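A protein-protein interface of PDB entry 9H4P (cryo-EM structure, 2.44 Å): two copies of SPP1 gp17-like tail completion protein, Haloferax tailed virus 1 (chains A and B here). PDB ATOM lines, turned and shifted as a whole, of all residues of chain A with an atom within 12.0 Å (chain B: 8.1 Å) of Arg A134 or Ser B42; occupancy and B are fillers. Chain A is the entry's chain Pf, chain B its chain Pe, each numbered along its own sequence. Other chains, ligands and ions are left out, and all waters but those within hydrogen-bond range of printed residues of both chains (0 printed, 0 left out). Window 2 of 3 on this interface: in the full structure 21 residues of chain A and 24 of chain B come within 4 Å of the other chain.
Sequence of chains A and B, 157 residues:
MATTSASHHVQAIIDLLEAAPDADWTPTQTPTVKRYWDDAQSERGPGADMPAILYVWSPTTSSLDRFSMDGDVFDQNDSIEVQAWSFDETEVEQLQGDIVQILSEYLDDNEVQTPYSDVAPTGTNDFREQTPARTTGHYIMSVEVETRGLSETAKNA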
ATOM      1  N   PHE A  87      -4.673   8.161  -5.421  1.00  0.00           N
ATOM      2  CA  PHE A  87      -4.356   7.288  -6.547  1.00  0.00           C
ATOM      3  C   PHE A  87      -4.203   8.057  -7.866  1.00  0.00           C
ATOM      4  O   PHE A  87      -3.725   7.484  -8.846  1.00  0.00           O
ATOM      5  CB  PHE A  87      -5.396   6.172  -6.680  1.00  0.00           C
ATOM      6  CG  PHE A  87      -5.399   5.159  -5.563  1.00  0.00           C
ATOM      7  CD1 PHE A  87      -4.285   4.365  -5.323  1.00  0.00           C
ATOM      8  CD2 PHE A  87      -6.517   4.988  -4.759  1.00  0.00           C
ATOM      9  CE1 PHE A  87      -4.282   3.434  -4.294  1.00  0.00           C
ATOM     10  CE2 PHE A  87      -6.515   4.053  -3.733  1.00  0.00           C
ATOM     11  CZ  PHE A  87      -5.399   3.277  -3.503  1.00  0.00           C
ATOM     12  N   GLU A  89      -2.391  10.909  -9.941  1.00  0.00           N
ATOM     13  CA  GLU A  89      -1.129  11.637 -10.061  1.00  0.00           C
ATOM     14  C   GLU A  89      -1.315  13.129 -10.364  1.00  0.00           C
ATOM     15  O   GLU A  89      -0.390  13.911 -10.142  1.00  0.00           O
ATOM     16  CB  GLU A  89      -0.260  10.989 -11.143  1.00  0.00           C
ATOM     17  CG  GLU A  89      -0.991  10.752 -12.459  1.00  0.00           C
ATOM     18  CD  GLU A  89      -0.137  10.778 -13.711  1.00  0.00           C
ATOM     19  OE1 GLU A  89       0.978  10.238 -13.678  1.00  0.00           O
ATOM     20  OE2 GLU A  89      -0.602  11.323 -14.724  1.00  0.00           O
ATOM     21  N   ARG A 128       6.186  11.628  -6.553  1.00  0.00           N
ATOM     22  CA  ARG A 128       5.515  10.774  -7.529  1.00  0.00           C
ATOM     23  C   ARG A 128       6.485   9.794  -8.195  1.00  0.00           C
ATOM     24  O   ARG A 128       6.059   8.718  -8.615  1.00  0.00           O
ATOM     25  CB  ARG A 128       4.770  11.608  -8.575  1.00  0.00           C
ATOM     26  CG  ARG A 128       3.516  12.277  -8.028  1.00  0.00           C
ATOM     27  CD  ARG A 128       2.832  13.208  -9.013  1.00  0.00           C
ATOM     28  NE  ARG A 128       3.684  14.341  -9.364  1.00  0.00           N
ATOM     29  CZ  ARG A 128       3.359  15.333 -10.191  1.00  0.00           C
ATOM     30  NH1 ARG A 128       4.230  16.299 -10.426  1.00  0.00           N
ATOM     31  NH2 ARG A 128       2.173  15.366 -10.775  1.00  0.00           N
ATOM     32  N   GLU A 129       7.779  10.161  -8.258  1.00  0.00           N
ATOM     33  CA  GLU A 129       8.832   9.320  -8.817  1.00  0.00           C
ATOM     34  C   GLU A 129       9.002   8.009  -8.036  1.00  0.00           C
ATOM     35  O   GLU A 129       9.567   7.055  -8.571  1.00  0.00           O
ATOM     36  CB  GLU A 129      10.148  10.097  -8.965  1.00  0.00           C
ATOM     37  CG  GLU A 129      10.884  10.360  -7.658  1.00  0.00           C
ATOM     38  CD  GLU A 129      10.419  11.535  -6.816  1.00  0.00           C
ATOM     39  OE1 GLU A 129       9.384  12.139  -7.147  1.00  0.00           O
ATOM     40  OE2 GLU A 129      11.107  11.850  -5.831  1.00  0.00           O
ATOM     41  N   GLN A 130       8.496   7.957  -6.793  1.00  0.00           N
ATOM     42  CA  GLN A 130       8.662   6.804  -5.915  1.00  0.00           C
ATOM     43  C   GLN A 130       7.603   5.725  -6.150  1.00  0.00           C
ATOM     44  O   GLN A 130       7.865   4.557  -5.862  1.00  0.00           O
ATOM     45  CB  GLN A 130       8.654   7.235  -4.447  1.00  0.00           C
ATOM     46  CG  GLN A 130       9.740   8.248  -4.117  1.00  0.00           C
ATOM     47  CD  GLN A 130       9.966   8.412  -2.635  1.00  0.00           C
ATOM     48  OE1 GLN A 130       9.061   8.252  -1.820  1.00  0.00           O
ATOM     49  NE2 GLN A 130      11.192   8.748  -2.271  1.00  0.00           N
ATOM     50  N   THR A 131       6.416   6.112  -6.643  1.00  0.00           N
ATOM     51  CA  THR A 131       5.292   5.197  -6.809  1.00  0.00           C
ATOM     52  C   THR A 131       5.609   4.185  -7.915  1.00  0.00           C
ATOM     53  O   THR A 131       5.796   4.587  -9.066  1.00  0.00           O
ATOM     54  CB  THR A 131       3.992   5.970  -7.077  1.00  0.00           C
ATOM     55  OG1 THR A 131       3.793   6.902  -6.014  1.00  0.00           O
ATOM     56  CG2 THR A 131       2.772   5.079  -7.188  1.00  0.00           C
ATOM     57  N   PRO A 132       5.691   2.859  -7.620  1.00  0.00           N
ATOM     58  CA  PRO A 132       6.071   1.866  -8.632  1.00  0.00           C
ATOM     59  C   PRO A 132       4.926   1.575  -9.604  1.00  0.00           C
ATOM     60  O   PRO A 132       3.793   1.350  -9.178  1.00  0.00           O
ATOM     61  CB  PRO A 132       6.440   0.627  -7.799  1.00  0.00           C
ATOM     62  CG  PRO A 132       5.599   0.745  -6.543  1.00  0.00           C
ATOM     63  CD  PRO A 132       5.424   2.234  -6.310  1.00  0.00           C
ATOM     64  N   ALA A 133       5.239   1.548 -10.906  1.00  0.00           N
ATOM     65  CA  ALA A 133       4.251   1.727 -11.960  1.00  0.00           C
ATOM     66  C   ALA A 133       3.383   0.490 -12.202  1.00  0.00           C
ATOM     67  O   ALA A 133       2.320   0.627 -12.806  1.00  0.00           O
ATOM     68  CB  ALA A 133       4.922   2.191 -13.231  1.00  0.00           C
ATOM     69  N   ARG A 134       3.814  -0.705 -11.758  1.00  0.00           N
ATOM     70  CA  ARG A 134       3.057  -1.936 -11.990  1.00  0.00           C
ATOM     71  C   ARG A 134       1.759  -1.932 -11.187  1.00  0.00           C
ATOM     72  O   ARG A 134       0.679  -2.143 -11.740  1.00  0.00           O
ATOM     73  CB  ARG A 134       3.826  -3.197 -11.580  1.00  0.00           C
ATOM     74  CG  ARG A 134       5.136  -3.413 -12.315  1.00  0.00           C
ATOM     75  CD  ARG A 134       5.679  -4.815 -12.144  1.00  0.00           C
ATOM     76  NE  ARG A 134       7.040  -4.730 -12.640  1.00  0.00           N
ATOM     77  CZ  ARG A 134       7.406  -4.866 -13.909  1.00  0.00           C
ATOM     78  NH1 ARG A 134       8.676  -4.735 -14.232  1.00  0.00           N
ATOM     79  NH2 ARG A 134       6.523  -5.130 -14.854  1.00  0.00           N
ATOM     80  N   THR A 135       1.898  -1.718  -9.873  1.00  0.00           N
ATOM     81  CA  THR A 135       0.811  -1.737  -8.910  1.00  0.00           C
ATOM     82  C   THR A 135       0.083  -0.396  -8.940  1.00  0.00           C
ATOM     83  O   THR A 135       0.712   0.642  -9.152  1.00  0.00           O
ATOM     84  CB  THR A 135       1.365  -1.954  -7.493  1.00  0.00           C
ATOM     85  OG1 THR A 135       2.396  -1.001  -7.231  1.00  0.00           O
ATOM     86  CG2 THR A 135       1.917  -3.344  -7.270  1.00  0.00           C
ATOM     87  N   THR A 136      -1.241  -0.420  -8.727  1.00  0.00           N
ATOM     88  CA  THR A 136      -1.904   0.772  -8.226  1.00  0.00           C
ATOM     89  C   THR A 136      -1.396   1.004  -6.805  1.00  0.00           C
ATOM     90  O   THR A 136      -1.264   0.061  -6.026  1.00  0.00           O
ATOM     91  CB  THR A 136      -3.434   0.699  -8.346  1.00  0.00           C
ATOM     92  OG1 THR A 136      -3.976   2.008  -8.171  1.00  0.00           O
ATOM     93  CG2 THR A 136      -4.080  -0.247  -7.357  1.00  0.00           C
ATOM     94  N   GLY A 137      -1.079   2.260  -6.497  1.00  0.00           N
ATOM     95  CA  GLY A 137      -0.556   2.665  -5.205  1.00  0.00           C
ATOM     96  C   GLY A 137      -0.542   4.185  -5.139  1.00  0.00           C
ATOM     97  O   GLY A 137      -0.573   4.836  -6.181  1.00  0.00           O
ATOM     98  N   HIS A 138      -0.494   4.741  -3.927  1.00  0.00           N
ATOM     99  CA  HIS A 138      -0.682   6.173  -3.760  1.00  0.00           C
ATOM    100  C   HIS A 138       0.479   6.956  -4.358  1.00  0.00           C
ATOM    101  O   HIS A 138       1.643   6.629  -4.134  1.00  0.00           O
ATOM    102  CB  HIS A 138      -0.888   6.520  -2.285  1.00  0.00           C
ATOM    103  CG  HIS A 138      -2.064   5.810  -1.714  1.00  0.00           C
ATOM    104  ND1 HIS A 138      -1.954   4.631  -1.003  1.00  0.00           N
ATOM    105  CD2 HIS A 138      -3.381   6.077  -1.806  1.00  0.00           C
ATOM    106  CE1 HIS A 138      -3.155   4.219  -0.655  1.00  0.00           C
ATOM    107  NE2 HIS A 138      -4.045   5.090  -1.135  1.00  0.00           N
ATOM    108  N   TYR A 139       0.119   7.990  -5.124  1.00  0.00           N
ATOM    109  CA  TYR A 139       0.996   9.114  -5.407  1.00  0.00           C
ATOM    110  C   TYR A 139       0.999  10.038  -4.191  1.00  0.00           C
ATOM    111  O   TYR A 139      -0.029  10.194  -3.532  1.00  0.00           O
ATOM    112  CB  TYR A 139       0.550   9.810  -6.696  1.00  0.00           C
ATOM    113  CG  TYR A 139       0.696   8.930  -7.912  1.00  0.00           C
ATOM    114  CD1 TYR A 139       1.951   8.692  -8.455  1.00  0.00           C
ATOM    115  CD2 TYR A 139      -0.395   8.293  -8.490  1.00  0.00           C
ATOM    116  CE1 TYR A 139       2.119   7.864  -9.553  1.00  0.00           C
ATOM    117  CE2 TYR A 139      -0.244   7.461  -9.590  1.00  0.00           C
ATOM    118  CZ  TYR A 139       1.018   7.245 -10.120  1.00  0.00           C
ATOM    119  OH  TYR A 139       1.177   6.434 -11.205  1.00  0.00           O
ATOM    120  N   TRP B  37       8.028   8.153 -13.382  1.00  0.00           N
ATOM    121  CA  TRP B  37       7.093   7.164 -12.859  1.00  0.00           C
ATOM    122  C   TRP B  37       6.173   6.569 -13.935  1.00  0.00           C
ATOM    123  O   TRP B  37       5.291   5.779 -13.594  1.00  0.00           O
ATOM    124  CB  TRP B  37       6.304   7.753 -11.674  1.00  0.00           C
ATOM    125  CG  TRP B  37       5.405   8.908 -12.007  1.00  0.00           C
ATOM    126  CD1 TRP B  37       4.107   8.818 -12.414  1.00  0.00           C
ATOM    127  CD2 TRP B  37       5.708  10.324 -11.947  1.00  0.00           C
ATOM    128  NE1 TRP B  37       3.586  10.067 -12.620  1.00  0.00           N
ATOM    129  CE2 TRP B  37       4.538  11.014 -12.341  1.00  0.00           C
ATOM    130  CE3 TRP B  37       6.841  11.088 -11.612  1.00  0.00           C
ATOM    131  CZ2 TRP B  37       4.475  12.412 -12.405  1.00  0.00           C
ATOM    132  CZ3 TRP B  37       6.779  12.466 -11.677  1.00  0.00           C
ATOM    133  CH2 TRP B  37       5.609  13.121 -12.071  1.00  0.00           C
ATOM    134  N   ASP B  38       6.383   6.909 -15.220  1.00  0.00           N
ATOM    135  CA  ASP B  38       5.578   6.358 -16.308  1.00  0.00           C
ATOM    136  C   ASP B  38       5.859   4.866 -16.524  1.00  0.00           C
ATOM    137  O   ASP B  38       4.972   4.142 -16.977  1.00  0.00           O
ATOM    138  CB  ASP B  38       5.759   7.133 -17.620  1.00  0.00           C
ATOM    139  CG  ASP B  38       5.088   8.496 -17.684  1.00  0.00           C
ATOM    140  OD1 ASP B  38       4.188   8.763 -16.866  1.00  0.00           O
ATOM    141  OD2 ASP B  38       5.465   9.276 -18.572  1.00  0.00           O
ATOM    142  N   ASP B  39       7.086   4.413 -16.204  1.00  0.00           N
ATOM    143  CA  ASP B  39       7.555   3.055 -16.478  1.00  0.00           C
ATOM    144  C   ASP B  39       7.981   2.346 -15.187  1.00  0.00           C
ATOM    145  O   ASP B  39       8.502   2.987 -14.275  1.00  0.00           O
ATOM    146  CB  ASP B  39       8.740   3.060 -17.452  1.00  0.00           C
ATOM    147  CG  ASP B  39       8.462   3.626 -18.836  1.00  0.00           C
ATOM    148  OD1 ASP B  39       7.285   3.660 -19.243  1.00  0.00           O
ATOM    149  OD2 ASP B  39       9.435   4.010 -19.508  1.00  0.00           O
ATOM    150  N   ALA B  40       7.778   1.018 -15.128  1.00  0.00           N
ATOM    151  CA  ALA B  40       8.287   0.176 -14.049  1.00  0.00           C
ATOM    152  C   ALA B  40       9.795  -0.023 -14.229  1.00  0.00           C
ATOM    153  O   ALA B  40      10.294   0.113 -15.346  1.00  0.00           O
ATOM    154  CB  ALA B  40       7.543  -1.137 -14.032  1.00  0.00           C
ATOM    155  N   GLN B  41      10.512  -0.354 -13.142  1.00  0.00           N
ATOM    156  CA  GLN B  41      11.974  -0.343 -13.119  1.00  0.00           C
ATOM    157  C   GLN B  41      12.592  -1.313 -14.134  1.00  0.00           C
ATOM    158  O   GLN B  41      13.534  -0.936 -14.829  1.00  0.00           O
ATOM    159  CB  GLN B  41      12.504  -0.564 -11.697  1.00  0.00           C
ATOM    160  CG  GLN B  41      14.021  -0.500 -11.559  1.00  0.00           C
ATOM    161  CD  GLN B  41      14.607   0.856 -11.865  1.00  0.00           C
ATOM    162  OE1 GLN B  41      14.761   1.246 -13.020  1.00  0.00           O
ATOM    163  NE2 GLN B  41      14.954   1.590 -10.822  1.00  0.00           N
ATOM    164  N   SER B  42      12.078  -2.553 -14.209  1.00  0.00           N
ATOM    165  CA  SER B  42      12.606  -3.573 -15.112  1.00  0.00           C
ATOM    166  C   SER B  42      12.362  -3.208 -16.579  1.00  0.00           C
ATOM    167  O   SER B  42      13.100  -3.659 -17.453  1.00  0.00           O
ATOM    168  CB  SER B  42      12.066  -4.954 -14.798  1.00  0.00           C
ATOM    169  OG  SER B  42      12.297  -5.311 -13.442  1.00  0.00           O
ATOM    170  N   GLU B  43      11.316  -2.402 -16.829  1.00  0.00           N
ATOM    171  CA  GLU B  43      10.957  -1.913 -18.153  1.00  0.00           C
ATOM    172  C   GLU B  43      11.681  -0.603 -18.484  1.00  0.00           C
ATOM    173  O   GLU B  43      11.665  -0.196 -19.643  1.00  0.00           O
ATOM    174  CB  GLU B  43       9.442  -1.700 -18.260  1.00  0.00           C
ATOM    175  CG  GLU B  43       8.660  -2.925 -18.707  1.00  0.00           C
ATOM    176  CD  GLU B  43       8.237  -3.888 -17.611  1.00  0.00           C
ATOM    177  OE1 GLU B  43       9.113  -4.384 -16.887  1.00  0.00           O
ATOM    178  OE2 GLU B  43       7.031  -4.144 -17.490  1.00  0.00           O
ATOM    179  N   ARG B  44      12.305   0.053 -17.488  1.00  0.00           N
ATOM    180  CA  ARG B  44      12.874   1.391 -17.639  1.00  0.00           C
ATOM    181  C   ARG B  44      14.031   1.400 -18.643  1.00  0.00           C
ATOM    182  O   ARG B  44      14.813   0.452 -18.703  1.00  0.00           O
ATOM    183  CB  ARG B  44      13.238   1.978 -16.270  1.00  0.00           C
ATOM    184  CG  ARG B  44      13.639   3.444 -16.308  1.00  0.00           C
ATOM    185  CD  ARG B  44      13.775   4.104 -14.950  1.00  0.00           C
ATOM    186  NE  ARG B  44      12.498   4.512 -14.378  1.00  0.00           N
ATOM    187  CZ  ARG B  44      11.991   4.095 -13.218  1.00  0.00           C
ATOM    188  NH1 ARG B  44      10.816   4.544 -12.814  1.00  0.00           N
ATOM    189  NH2 ARG B  44      12.649   3.240 -12.458  1.00  0.00           N
ATOM    190  N   GLY B  45      14.123   2.496 -19.414  1.00  0.00           N
ATOM    191  CA  GLY B  45      15.030   2.623 -20.545  1.00  0.00           C
ATOM    192  C   GLY B  45      14.423   2.060 -21.831  1.00  0.00           C
ATOM    193  O   GLY B  45      13.481   1.268 -21.770  1.00  0.00           O
ATOM    194  N   PRO B  46      14.935   2.447 -23.028  1.00  0.00           N
ATOM    195  CA  PRO B  46      14.396   1.954 -24.300  1.00  0.00           C
ATOM    196  C   PRO B  46      14.758   0.491 -24.552  1.00  0.00           C
ATOM    197  O   PRO B  46      15.727  -0.013 -23.992  1.00  0.00           O
ATOM    198  CB  PRO B  46      15.090   2.842 -25.346  1.00  0.00           C
ATOM    199  CG  PRO B  46      16.398   3.243 -24.695  1.00  0.00           C
ATOM    200  CD  PRO B  46      16.062   3.379 -23.225  1.00  0.00           C
ATOM    201  N   TRP B  85      18.375   7.887 -21.346  1.00  0.00           N
ATOM    202  CA  TRP B  85      18.694   6.461 -21.364  1.00  0.00           C
ATOM    203  C   TRP B  85      18.812   5.974 -22.810  1.00  0.00           C
ATOM    204  O   TRP B  85      17.909   6.227 -23.609  1.00  0.00           O
ATOM    205  CB  TRP B  85      17.613   5.634 -20.636  1.00  0.00           C
ATOM    206  CG  TRP B  85      17.489   5.756 -19.142  1.00  0.00           C
ATOM    207  CD1 TRP B  85      17.309   6.902 -18.420  1.00  0.00           C
ATOM    208  CD2 TRP B  85      17.442   4.675 -18.180  1.00  0.00           C
ATOM    209  NE1 TRP B  85      17.189   6.612 -17.086  1.00  0.00           N
ATOM    210  CE2 TRP B  85      17.263   5.254 -16.902  1.00  0.00           C
ATOM    211  CE3 TRP B  85      17.548   3.276 -18.256  1.00  0.00           C
ATOM    212  CZ2 TRP B  85      17.191   4.480 -15.737  1.00  0.00           C
ATOM    213  CZ3 TRP B  85      17.474   2.513 -17.106  1.00  0.00           C
ATOM    214  CH2 TRP B  85      17.298   3.110 -15.856  1.00  0.00           C
ATOM    215  N   HIS B 138      21.810  -0.200 -20.339  1.00  0.00           N
ATOM    216  CA  HIS B 138      21.636   1.215 -20.629  1.00  0.00           C
ATOM    217  C   HIS B 138      22.805   2.037 -20.100  1.00  0.00           C
ATOM    218  O   HIS B 138      23.262   1.830 -18.978  1.00  0.00           O
ATOM    219  CB  HIS B 138      20.316   1.735 -20.053  1.00  0.00           C
ATOM    220  CG  HIS B 138      19.134   1.043 -20.636  1.00  0.00           C
ATOM    221  ND1 HIS B 138      18.420   0.086 -19.945  1.00  0.00           N
ATOM    222  CD2 HIS B 138      18.571   1.133 -21.857  1.00  0.00           C
ATOM    223  CE1 HIS B 138      17.454  -0.372 -20.711  1.00  0.00           C
ATOM    224  NE2 HIS B 138      17.525   0.257 -21.887  1.00  0.00           N
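Of the printed residues of chain B, Arg A128 touches Trp B37 (3.2 Å).
Printed residues of chain B within 4 Å of Glu A129: Trp B37 (3.6 Å).
Gln A130 touches none of the printed residues of chain B.
Thr A131 touches none of the printed residues of chain B.
Ala A133 touches three residues of chain B.
Printed residues of chain B within 4 Å of Arg A134: Ala B40, Ser B42 and Glu B43.
Ala B40 touches just these residues of chain A: Ala A133 and Arg A134.
Ser B42 touches one residue of chain A.
No residue of chain A comes within 4 Å of Gly B45.
The nearest residue of chain A that does not touch Ser B42 is Ala A133 (8.6 Å).
OE1 of Glu A89 is in hydrogen-bond range of NE1 of Trp B37, at 2.8 Å.
The side-chain carboxylate of Glu B43 is in salt-bridge range of the guanidinium group of Arg A134 (2.7 Å).
1 position is printed for both chains.
Among the printed residues, pairs that only touch across the chains: Arg A128 with Trp B37 (3.2 Å), Glu A129 with Trp B37 (3.6 Å), Ala A133 with Trp B37 (3.6 Å), Ala A133 with Asp B39 (3.6 Å), Ala A133 with Ala B40 (3.6 Å), Arg A134 with Ala B40 (3.7 Å), Arg A134 with Ser B42 (3.4 Å) and Tyr A139 with Trp B37 (3.6 Å).
O of Asp B39 is in hydrogen-bond range of NH1 of Arg B44 (3.1 Å).
O of Glu A89 lies within hydrogen-bond range of NH2 of Arg A128, 3.0 Å away.
Of the 14 printed residues of chain A, 6 touch a printed residue of chain B.
Of the 12 printed residues of chain B, 5 touch a printed residue of chain A.
Among the printed residues, Asp or Glu carboxylates within 4 Å of a Lys or Arg side-chain nitrogen of the other chain: Arg A134 with Glu B43.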
